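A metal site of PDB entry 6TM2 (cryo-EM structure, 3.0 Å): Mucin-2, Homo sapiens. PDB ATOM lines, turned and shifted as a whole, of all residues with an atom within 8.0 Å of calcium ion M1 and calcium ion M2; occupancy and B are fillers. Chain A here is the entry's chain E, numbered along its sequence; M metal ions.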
ATOM      1  N   ILE A 112     -14.739   8.658  -2.836  1.00  0.00           N
ATOM      2  CA  ILE A 112     -13.699   8.935  -3.820  1.00  0.00           C
ATOM      3  C   ILE A 112     -13.149  10.318  -3.533  1.00  0.00           C
ATOM      4  O   ILE A 112     -13.810  11.324  -3.805  1.00  0.00           O
ATOM      5  CB  ILE A 112     -14.233   8.830  -5.258  1.00  0.00           C
ATOM      6  CG1 ILE A 112     -14.750   7.418  -5.531  1.00  0.00           C
ATOM      7  CG2 ILE A 112     -13.142   9.169  -6.249  1.00  0.00           C
ATOM      8  CD1 ILE A 112     -15.530   7.306  -6.814  1.00  0.00           C
ATOM      9  N   ASN A 113     -11.944  10.369  -2.986  1.00  0.00           N
ATOM     10  CA  ASN A 113     -11.214  11.626  -2.772  1.00  0.00           C
ATOM     11  C   ASN A 113      -9.954  11.530  -3.619  1.00  0.00           C
ATOM     12  O   ASN A 113      -8.895  11.121  -3.129  1.00  0.00           O
ATOM     13  CB  ASN A 113     -10.894  11.838  -1.296  1.00  0.00           C
ATOM     14  CG  ASN A 113     -10.425  13.247  -0.998  1.00  0.00           C
ATOM     15  OD1 ASN A 113     -10.433  14.124  -1.870  1.00  0.00           O
ATOM     16  ND2 ASN A 113      -9.950  13.459   0.214  1.00  0.00           N
ATOM     17  N   GLU A 114     -10.058  11.908  -4.883  1.00  0.00           N
ATOM     18  CA  GLU A 114      -8.959  11.776  -5.830  1.00  0.00           C
ATOM     19  C   GLU A 114      -8.429  13.132  -6.286  1.00  0.00           C
ATOM     20  O   GLU A 114      -7.736  13.204  -7.300  1.00  0.00           O
ATOM     21  CB  GLU A 114      -9.389  10.937  -7.027  1.00  0.00           C
ATOM     22  N   ASP A 115      -8.728  14.193  -5.552  1.00  0.00           N
ATOM     23  CA  ASP A 115      -8.295  15.525  -5.926  1.00  0.00           C
ATOM     24  C   ASP A 115      -8.247  16.363  -4.650  1.00  0.00           C
ATOM     25  O   ASP A 115      -8.857  16.012  -3.635  1.00  0.00           O
ATOM     26  CB  ASP A 115      -9.244  16.134  -6.968  1.00  0.00           C
ATOM     27  CG  ASP A 115      -8.661  17.353  -7.654  1.00  0.00           C
ATOM     28  OD1 ASP A 115      -7.522  17.755  -7.323  1.00  0.00           O
ATOM     29  OD2 ASP A 115      -9.340  17.908  -8.550  1.00  0.00           O
ATOM     30  N   HIS A 116      -7.488  17.450  -4.694  1.00  0.00           N
ATOM     31  CA  HIS A 116      -7.264  18.293  -3.540  1.00  0.00           C
ATOM     32  C   HIS A 116      -7.234  19.749  -3.969  1.00  0.00           C
ATOM     33  O   HIS A 116      -6.959  20.054  -5.130  1.00  0.00           O
ATOM     34  CB  HIS A 116      -5.950  17.932  -2.829  1.00  0.00           C
ATOM     35  CG  HIS A 116      -5.957  16.560  -2.230  1.00  0.00           C
ATOM     36  ND1 HIS A 116      -6.610  16.272  -1.058  1.00  0.00           N
ATOM     37  CD2 HIS A 116      -5.432  15.394  -2.669  1.00  0.00           C
ATOM     38  CE1 HIS A 116      -6.464  14.988  -0.781  1.00  0.00           C
ATOM     39  NE2 HIS A 116      -5.757  14.432  -1.742  1.00  0.00           N
ATOM     40  N   PRO A 117      -7.547  20.676  -3.059  1.00  0.00           N
ATOM     41  CA  PRO A 117      -7.400  22.101  -3.403  1.00  0.00           C
ATOM     42  C   PRO A 117      -5.955  22.567  -3.438  1.00  0.00           C
ATOM     43  O   PRO A 117      -5.593  23.394  -4.277  1.00  0.00           O
ATOM     44  CB  PRO A 117      -8.201  22.804  -2.301  1.00  0.00           C
ATOM     45  CG  PRO A 117      -9.144  21.782  -1.806  1.00  0.00           C
ATOM     46  CD  PRO A 117      -8.403  20.498  -1.877  1.00  0.00           C
ATOM     47  N   SER A 118      -5.108  22.046  -2.541  1.00  0.00           N
ATOM     48  CA  SER A 118      -3.706  22.433  -2.469  1.00  0.00           C
ATOM     49  C   SER A 118      -2.807  21.543  -3.329  1.00  0.00           C
ATOM     50  O   SER A 118      -1.610  21.446  -3.049  1.00  0.00           O
ATOM     51  CB  SER A 118      -3.229  22.418  -1.022  1.00  0.00           C
ATOM     52  OG  SER A 118      -1.860  22.762  -0.921  1.00  0.00           O
ATOM     53  N   SER A 119      -3.366  20.893  -4.341  1.00  0.00           N
ATOM     54  CA  SER A 119      -2.607  20.095  -5.302  1.00  0.00           C
ATOM     55  C   SER A 119      -3.426  20.026  -6.580  1.00  0.00           C
ATOM     56  O   SER A 119      -4.519  20.576  -6.680  1.00  0.00           O
ATOM     57  CB  SER A 119      -2.289  18.696  -4.759  1.00  0.00           C
ATOM     58  OG  SER A 119      -1.410  18.771  -3.656  1.00  0.00           O
ATOM     59  N   GLY A 120      -2.885  19.329  -7.573  1.00  0.00           N
ATOM     60  CA  GLY A 120      -3.528  19.246  -8.863  1.00  0.00           C
ATOM     61  C   GLY A 120      -3.282  20.476  -9.704  1.00  0.00           C
ATOM     62  O   GLY A 120      -2.448  21.337  -9.384  1.00  0.00           O
ATOM     63  N   SER A 121      -4.015  20.561 -10.817  1.00  0.00           N
ATOM     64  CA  SER A 121      -3.884  21.705 -11.711  1.00  0.00           C
ATOM     65  C   SER A 121      -5.212  22.165 -12.288  1.00  0.00           C
ATOM     66  O   SER A 121      -5.209  22.969 -13.234  1.00  0.00           O
ATOM     67  CB  SER A 121      -2.916  21.369 -12.853  1.00  0.00           C
ATOM     68  OG  SER A 121      -1.604  21.155 -12.348  1.00  0.00           O
ATOM     69  N   ASP A 122      -6.347  21.703 -11.768  1.00  0.00           N
ATOM     70  CA  ASP A 122      -7.650  22.120 -12.259  1.00  0.00           C
ATOM     71  C   ASP A 122      -8.220  23.329 -11.536  1.00  0.00           C
ATOM     72  O   ASP A 122      -9.395  23.658 -11.747  1.00  0.00           O
ATOM     73  CB  ASP A 122      -8.638  20.936 -12.197  1.00  0.00           C
ATOM     74  CG  ASP A 122      -8.780  20.351 -10.803  1.00  0.00           C
ATOM     75  OD1 ASP A 122      -8.060  20.777  -9.871  1.00  0.00           O
ATOM     76  OD2 ASP A 122      -9.619  19.451 -10.626  1.00  0.00           O
ATOM     77  N   ASP A 123      -7.409  23.979 -10.686  1.00  0.00           N
ATOM     78  CA  ASP A 123      -7.725  25.241  -9.999  1.00  0.00           C
ATOM     79  C   ASP A 123      -8.957  25.102  -9.112  1.00  0.00           C
ATOM     80  O   ASP A 123      -9.862  25.938  -9.111  1.00  0.00           O
ATOM     81  CB  ASP A 123      -7.885  26.383 -11.020  1.00  0.00           C
ATOM     82  CG  ASP A 123      -7.780  27.768 -10.388  1.00  0.00           C
ATOM     83  OD1 ASP A 123      -7.560  27.871  -9.173  1.00  0.00           O
ATOM     84  OD2 ASP A 123      -7.935  28.768 -11.132  1.00  0.00           O
ATOM     85  N   GLY A 124      -9.006  24.016  -8.335  1.00  0.00           N
ATOM     86  CA  GLY A 124     -10.167  23.765  -7.507  1.00  0.00           C
ATOM     87  C   GLY A 124     -10.252  22.332  -7.036  1.00  0.00           C
ATOM     88  O   GLY A 124      -9.265  21.778  -6.545  1.00  0.00           O
ATOM     89  N   ASP A 125     -11.421  21.713  -7.176  1.00  0.00           N
ATOM     90  CA  ASP A 125     -11.607  20.333  -6.723  1.00  0.00           C
ATOM     91  C   ASP A 125     -12.684  19.709  -7.598  1.00  0.00           C
ATOM     92  O   ASP A 125     -13.816  20.204  -7.630  1.00  0.00           O
ATOM     93  CB  ASP A 125     -11.997  20.286  -5.252  1.00  0.00           C
ATOM     94  CG  ASP A 125     -11.880  18.902  -4.653  1.00  0.00           C
ATOM     95  OD1 ASP A 125     -11.505  17.957  -5.371  1.00  0.00           O
ATOM     96  OD2 ASP A 125     -12.156  18.754  -3.458  1.00  0.00           O
ATOM     97  N   ARG A 126     -12.332  18.636  -8.297  1.00  0.00           N
ATOM     98  CA  ARG A 126     -13.259  17.964  -9.196  1.00  0.00           C
ATOM     99  C   ARG A 126     -13.143  16.462  -9.012  1.00  0.00           C
ATOM    100  O   ARG A 126     -12.046  15.908  -9.097  1.00  0.00           O
ATOM    101  CB  ARG A 126     -12.997  18.338 -10.657  1.00  0.00           C
ATOM    102  CG  ARG A 126     -13.338  19.780 -11.001  1.00  0.00           C
ATOM    103  CD  ARG A 126     -13.048  20.130 -12.443  1.00  0.00           C
ATOM    104  NE  ARG A 126     -13.373  21.529 -12.707  1.00  0.00           N
ATOM    105  CZ  ARG A 126     -13.168  22.130 -13.873  1.00  0.00           C
ATOM    106  NH1 ARG A 126     -12.638  21.462 -14.889  1.00  0.00           N
ATOM    107  NH2 ARG A 126     -13.489  23.409 -14.029  1.00  0.00           N
ATOM    108  N   GLU A 127     -14.272  15.804  -8.766  1.00  0.00           N
ATOM    109  CA  GLU A 127     -14.333  14.378  -8.490  1.00  0.00           C
ATOM    110  C   GLU A 127     -15.297  13.731  -9.471  1.00  0.00           C
ATOM    111  O   GLU A 127     -16.486  14.048  -9.469  1.00  0.00           O
ATOM    112  CB  GLU A 127     -14.779  14.119  -7.039  1.00  0.00           C
ATOM    113  CG  GLU A 127     -13.786  14.581  -5.997  1.00  0.00           C
ATOM    114  CD  GLU A 127     -12.525  13.752  -6.004  1.00  0.00           C
ATOM    115  OE1 GLU A 127     -12.594  12.546  -6.301  1.00  0.00           O
ATOM    116  OE2 GLU A 127     -11.455  14.315  -5.715  1.00  0.00           O
ATOM    117  N   ARG A 142     -20.232  15.352  -0.129  1.00  0.00           N
ATOM    118  CA  ARG A 142     -19.860  15.694   1.251  1.00  0.00           C
ATOM    119  C   ARG A 142     -18.419  16.169   1.309  1.00  0.00           C
ATOM    120  O   ARG A 142     -17.692  16.168   0.316  1.00  0.00           O
ATOM    121  CB  ARG A 142     -20.066  14.517   2.204  1.00  0.00           C
ATOM    122  CG  ARG A 142     -21.511  14.118   2.348  1.00  0.00           C
ATOM    123  CD  ARG A 142     -22.260  15.234   3.047  1.00  0.00           C
ATOM    124  NE  ARG A 142     -23.688  14.969   3.179  1.00  0.00           N
ATOM    125  CZ  ARG A 142     -24.228  14.342   4.211  1.00  0.00           C
ATOM    126  NH1 ARG A 142     -23.460  13.894   5.199  1.00  0.00           N
ATOM    127  NH2 ARG A 142     -25.535  14.148   4.255  1.00  0.00           N
ATOM    128  N   SER A 143     -18.015  16.585   2.504  1.00  0.00           N
ATOM    129  CA  SER A 143     -16.672  17.104   2.753  1.00  0.00           C
ATOM    130  C   SER A 143     -15.856  16.097   3.546  1.00  0.00           C
ATOM    131  O   SER A 143     -16.381  15.216   4.214  1.00  0.00           O
ATOM    132  CB  SER A 143     -16.720  18.423   3.523  1.00  0.00           C
ATOM    133  OG  SER A 143     -15.407  18.899   3.784  1.00  0.00           O
ATOM    134  N   VAL A 144     -14.537  16.252   3.466  1.00  0.00           N
ATOM    135  CA  VAL A 144     -13.638  15.293   4.066  1.00  0.00           C
ATOM    136  C   VAL A 144     -13.546  15.500   5.572  1.00  0.00           C
ATOM    137  O   VAL A 144     -13.796  14.575   6.363  1.00  0.00           O
ATOM    138  CB  VAL A 144     -12.255  15.378   3.412  1.00  0.00           C
ATOM    139  CG1 VAL A 144     -11.287  14.465   4.109  1.00  0.00           C
ATOM    140  CG2 VAL A 144     -12.363  15.006   1.969  1.00  0.00           C
ATOM    141  N   PHE A 166     -18.545  16.329  -9.840  1.00  0.00           N
ATOM    142  CA  PHE A 166     -18.403  17.432  -8.897  1.00  0.00           C
ATOM    143  C   PHE A 166     -17.451  18.460  -9.478  1.00  0.00           C
ATOM    144  O   PHE A 166     -16.418  18.111 -10.057  1.00  0.00           O
ATOM    145  CB  PHE A 166     -17.896  16.937  -7.548  1.00  0.00           C
ATOM    146  CG  PHE A 166     -17.740  18.011  -6.525  1.00  0.00           C
ATOM    147  CD1 PHE A 166     -18.842  18.561  -5.905  1.00  0.00           C
ATOM    148  CD2 PHE A 166     -16.486  18.486  -6.183  1.00  0.00           C
ATOM    149  CE1 PHE A 166     -18.712  19.561  -4.976  1.00  0.00           C
ATOM    150  CE2 PHE A 166     -16.342  19.482  -5.253  1.00  0.00           C
ATOM    151  CZ  PHE A 166     -17.454  20.024  -4.652  1.00  0.00           C
ATOM    152  N   CYS A 168     -15.700  22.269  -8.323  1.00  0.00           N
ATOM    153  CA  CYS A 168     -15.458  23.457  -7.522  1.00  0.00           C
ATOM    154  C   CYS A 168     -14.344  24.240  -8.197  1.00  0.00           C
ATOM    155  O   CYS A 168     -13.323  23.655  -8.583  1.00  0.00           O
ATOM    156  CB  CYS A 168     -15.073  23.112  -6.065  1.00  0.00           C
ATOM    157  SG  CYS A 168     -14.906  24.507  -4.914  1.00  0.00           S
ATOM    158  N   ASN A 170     -11.818  27.658  -7.852  1.00  0.00           N
ATOM    159  CA  ASN A 170     -11.289  28.629  -6.880  1.00  0.00           C
ATOM    160  C   ASN A 170     -11.639  30.063  -7.243  1.00  0.00           C
ATOM    161  O   ASN A 170     -11.681  30.922  -6.352  1.00  0.00           O
ATOM    162  CB  ASN A 170      -9.771  28.517  -6.743  1.00  0.00           C
ATOM    163  CG  ASN A 170      -9.339  27.304  -5.968  1.00  0.00           C
ATOM    164  OD1 ASN A 170      -9.960  26.937  -4.984  1.00  0.00           O
ATOM    165  ND2 ASN A 170      -8.240  26.701  -6.394  1.00  0.00           N
ATOM    166  N   TYR A 183     -12.922  23.805  -0.364  1.00  0.00           N
ATOM    167  CA  TYR A 183     -12.740  22.845   0.706  1.00  0.00           C
ATOM    168  C   TYR A 183     -12.429  21.494   0.071  1.00  0.00           C
ATOM    169  O   TYR A 183     -12.441  21.340  -1.156  1.00  0.00           O
ATOM    170  CB  TYR A 183     -13.970  22.801   1.605  1.00  0.00           C
ATOM    171  CG  TYR A 183     -14.229  24.092   2.358  1.00  0.00           C
ATOM    172  CD1 TYR A 183     -13.209  25.001   2.613  1.00  0.00           C
ATOM    173  CD2 TYR A 183     -15.513  24.451   2.732  1.00  0.00           C
ATOM    174  CE1 TYR A 183     -13.455  26.177   3.266  1.00  0.00           C
ATOM    175  CE2 TYR A 183     -15.770  25.633   3.367  1.00  0.00           C
ATOM    176  CZ  TYR A 183     -14.731  26.494   3.638  1.00  0.00           C
ATOM    177  OH  TYR A 183     -14.978  27.686   4.275  1.00  0.00           O
ATOM    178  N   ASP A 184     -12.143  20.495   0.881  1.00  0.00           N
ATOM    179  CA  ASP A 184     -11.776  19.184   0.388  1.00  0.00           C
ATOM    180  C   ASP A 184     -13.023  18.304   0.398  1.00  0.00           C
ATOM    181  O   ASP A 184     -13.593  18.059   1.470  1.00  0.00           O
ATOM    182  CB  ASP A 184     -10.658  18.590   1.238  1.00  0.00           C
ATOM    183  CG  ASP A 184     -10.003  17.387   0.600  1.00  0.00           C
ATOM    184  OD1 ASP A 184     -10.405  16.976  -0.508  1.00  0.00           O
ATOM    185  OD2 ASP A 184      -9.066  16.846   1.220  1.00  0.00           O
ATOM    186  N   TYR A 185     -13.443  17.849  -0.773  1.00  0.00           N
ATOM    187  CA  TYR A 185     -14.699  17.141  -0.951  1.00  0.00           C
ATOM    188  C   TYR A 185     -14.448  15.687  -1.349  1.00  0.00           C
ATOM    189  O   TYR A 185     -13.343  15.307  -1.730  1.00  0.00           O
ATOM    190  CB  TYR A 185     -15.546  17.844  -2.016  1.00  0.00           C
ATOM    191  CG  TYR A 185     -16.095  19.195  -1.614  1.00  0.00           C
ATOM    192  CD1 TYR A 185     -17.290  19.296  -0.917  1.00  0.00           C
ATOM    193  CD2 TYR A 185     -15.404  20.358  -1.898  1.00  0.00           C
ATOM    194  CE1 TYR A 185     -17.804  20.519  -0.561  1.00  0.00           C
ATOM    195  CE2 TYR A 185     -15.901  21.591  -1.533  1.00  0.00           C
ATOM    196  CZ  TYR A 185     -17.103  21.664  -0.868  1.00  0.00           C
ATOM    197  OH  TYR A 185     -17.604  22.882  -0.510  1.00  0.00           O
ATOM    198  N   LYS A 186     -15.507  14.892  -1.262  1.00  0.00           N
ATOM    199  CA  LYS A 186     -15.484  13.483  -1.610  1.00  0.00           C
ATOM    200  C   LYS A 186     -16.897  13.064  -1.982  1.00  0.00           C
ATOM    201  O   LYS A 186     -17.865  13.679  -1.554  1.00  0.00           O
ATOM    202  CB  LYS A 186     -14.932  12.638  -0.461  1.00  0.00           C
ATOM    203  CG  LYS A 186     -15.797  12.664   0.787  1.00  0.00           C
ATOM    204  CD  LYS A 186     -15.183  11.862   1.904  1.00  0.00           C
ATOM    205  CE  LYS A 186     -16.079  11.877   3.113  1.00  0.00           C
ATOM    206  NZ  LYS A 186     -15.499  11.083   4.222  1.00  0.00           N
ATOM    207  N   ILE A 187     -17.020  12.017  -2.820  1.00  0.00           N
ATOM    208  CA  ILE A 187     -18.315  11.616  -3.370  1.00  0.00           C
ATOM    209  C   ILE A 187     -18.507  10.102  -3.339  1.00  0.00           C
ATOM    210  O   ILE A 187     -17.555   9.319  -3.327  1.00  0.00           O
ATOM    211  CB  ILE A 187     -18.532  12.103  -4.830  1.00  0.00           C
ATOM    212  CG1 ILE A 187     -17.463  11.539  -5.756  1.00  0.00           C
ATOM    213  CG2 ILE A 187     -18.633  13.624  -4.913  1.00  0.00           C
ATOM    214  CD1 ILE A 187     -17.764  11.756  -7.225  1.00  0.00           C
HETATM  215 CA    CA M   1      -6.804  20.187  -7.758  1.00  0.00          CA
HETATM  216 CA    CA M   2     -11.318  16.236  -2.979  1.00  0.00          CA
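Residues that only touch calcium ion M1: Gly 120 (3.6 Å) and Gly 124 (3.2 Å).
Within 4 Å of calcium ion M1: Asp 115, His 116, Ser 119, Gly 120, Asp 122 and Gly 124.
The nearest printed residue that does not touch calcium ion M1 is Ser 121 (4.2 Å).
Calcium ion M1 is bound by OD1 of Asp 122 (2.5 Å), O of Ser 119 (2.6 Å), OD1 of Asp 115 (2.6 Å) and O of His 116 (2.6 Å).
The backbone NH (N) of Asp 115 sits at hydrogen-bond distance from the side-chain carboxylate (OE2) of Glu 127 (2.7 Å).
A ring nitrogen (ND1) of His 116 lies within hydrogen-bond range of the side-chain carboxylate of Asp 184.
The backbone carbonyl oxygen of Asp 125 lies within hydrogen-bond range of the backbone NH of Cys 168 (2.9 Å).
O of Asp 184 sits at hydrogen-bond distance from N of Val 144 (2.9 Å).
The side-chain hydroxyl (OG) of Ser 143 lies within hydrogen-bond range of the backbone carbonyl oxygen (O) of Asp 184 (3.1 Å).
N of Gly 124 sits close to ND2 of Asn 170 (3.4 Å).
OE2 of Glu 127 is in hydrogen-bond range of N of Glu 114.
The backbone carbonyl oxygen (O) of Glu 127 is in hydrogen-bond range of the backbone NH (N) of Phe 166.
Calcium ion M2 is bound by OD1 of Asn 113 (2.5 Å), O of Tyr 185 (2.6 Å), O of Asp 115 (2.6 Å), OD2 of Asp 125 (2.7 Å) and OD1 of Asp 184 (2.7 Å).
Slightly farther from calcium ion M2 lies the side-chain carboxylate (OD1) of Asp 125 (3.0 Å).
Glu 127 touches calcium ion M2.
Within 4 Å of calcium ion M2: Asn 113, Asp 115, Asp 125, Glu 127, Asp 184 and Tyr 185.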
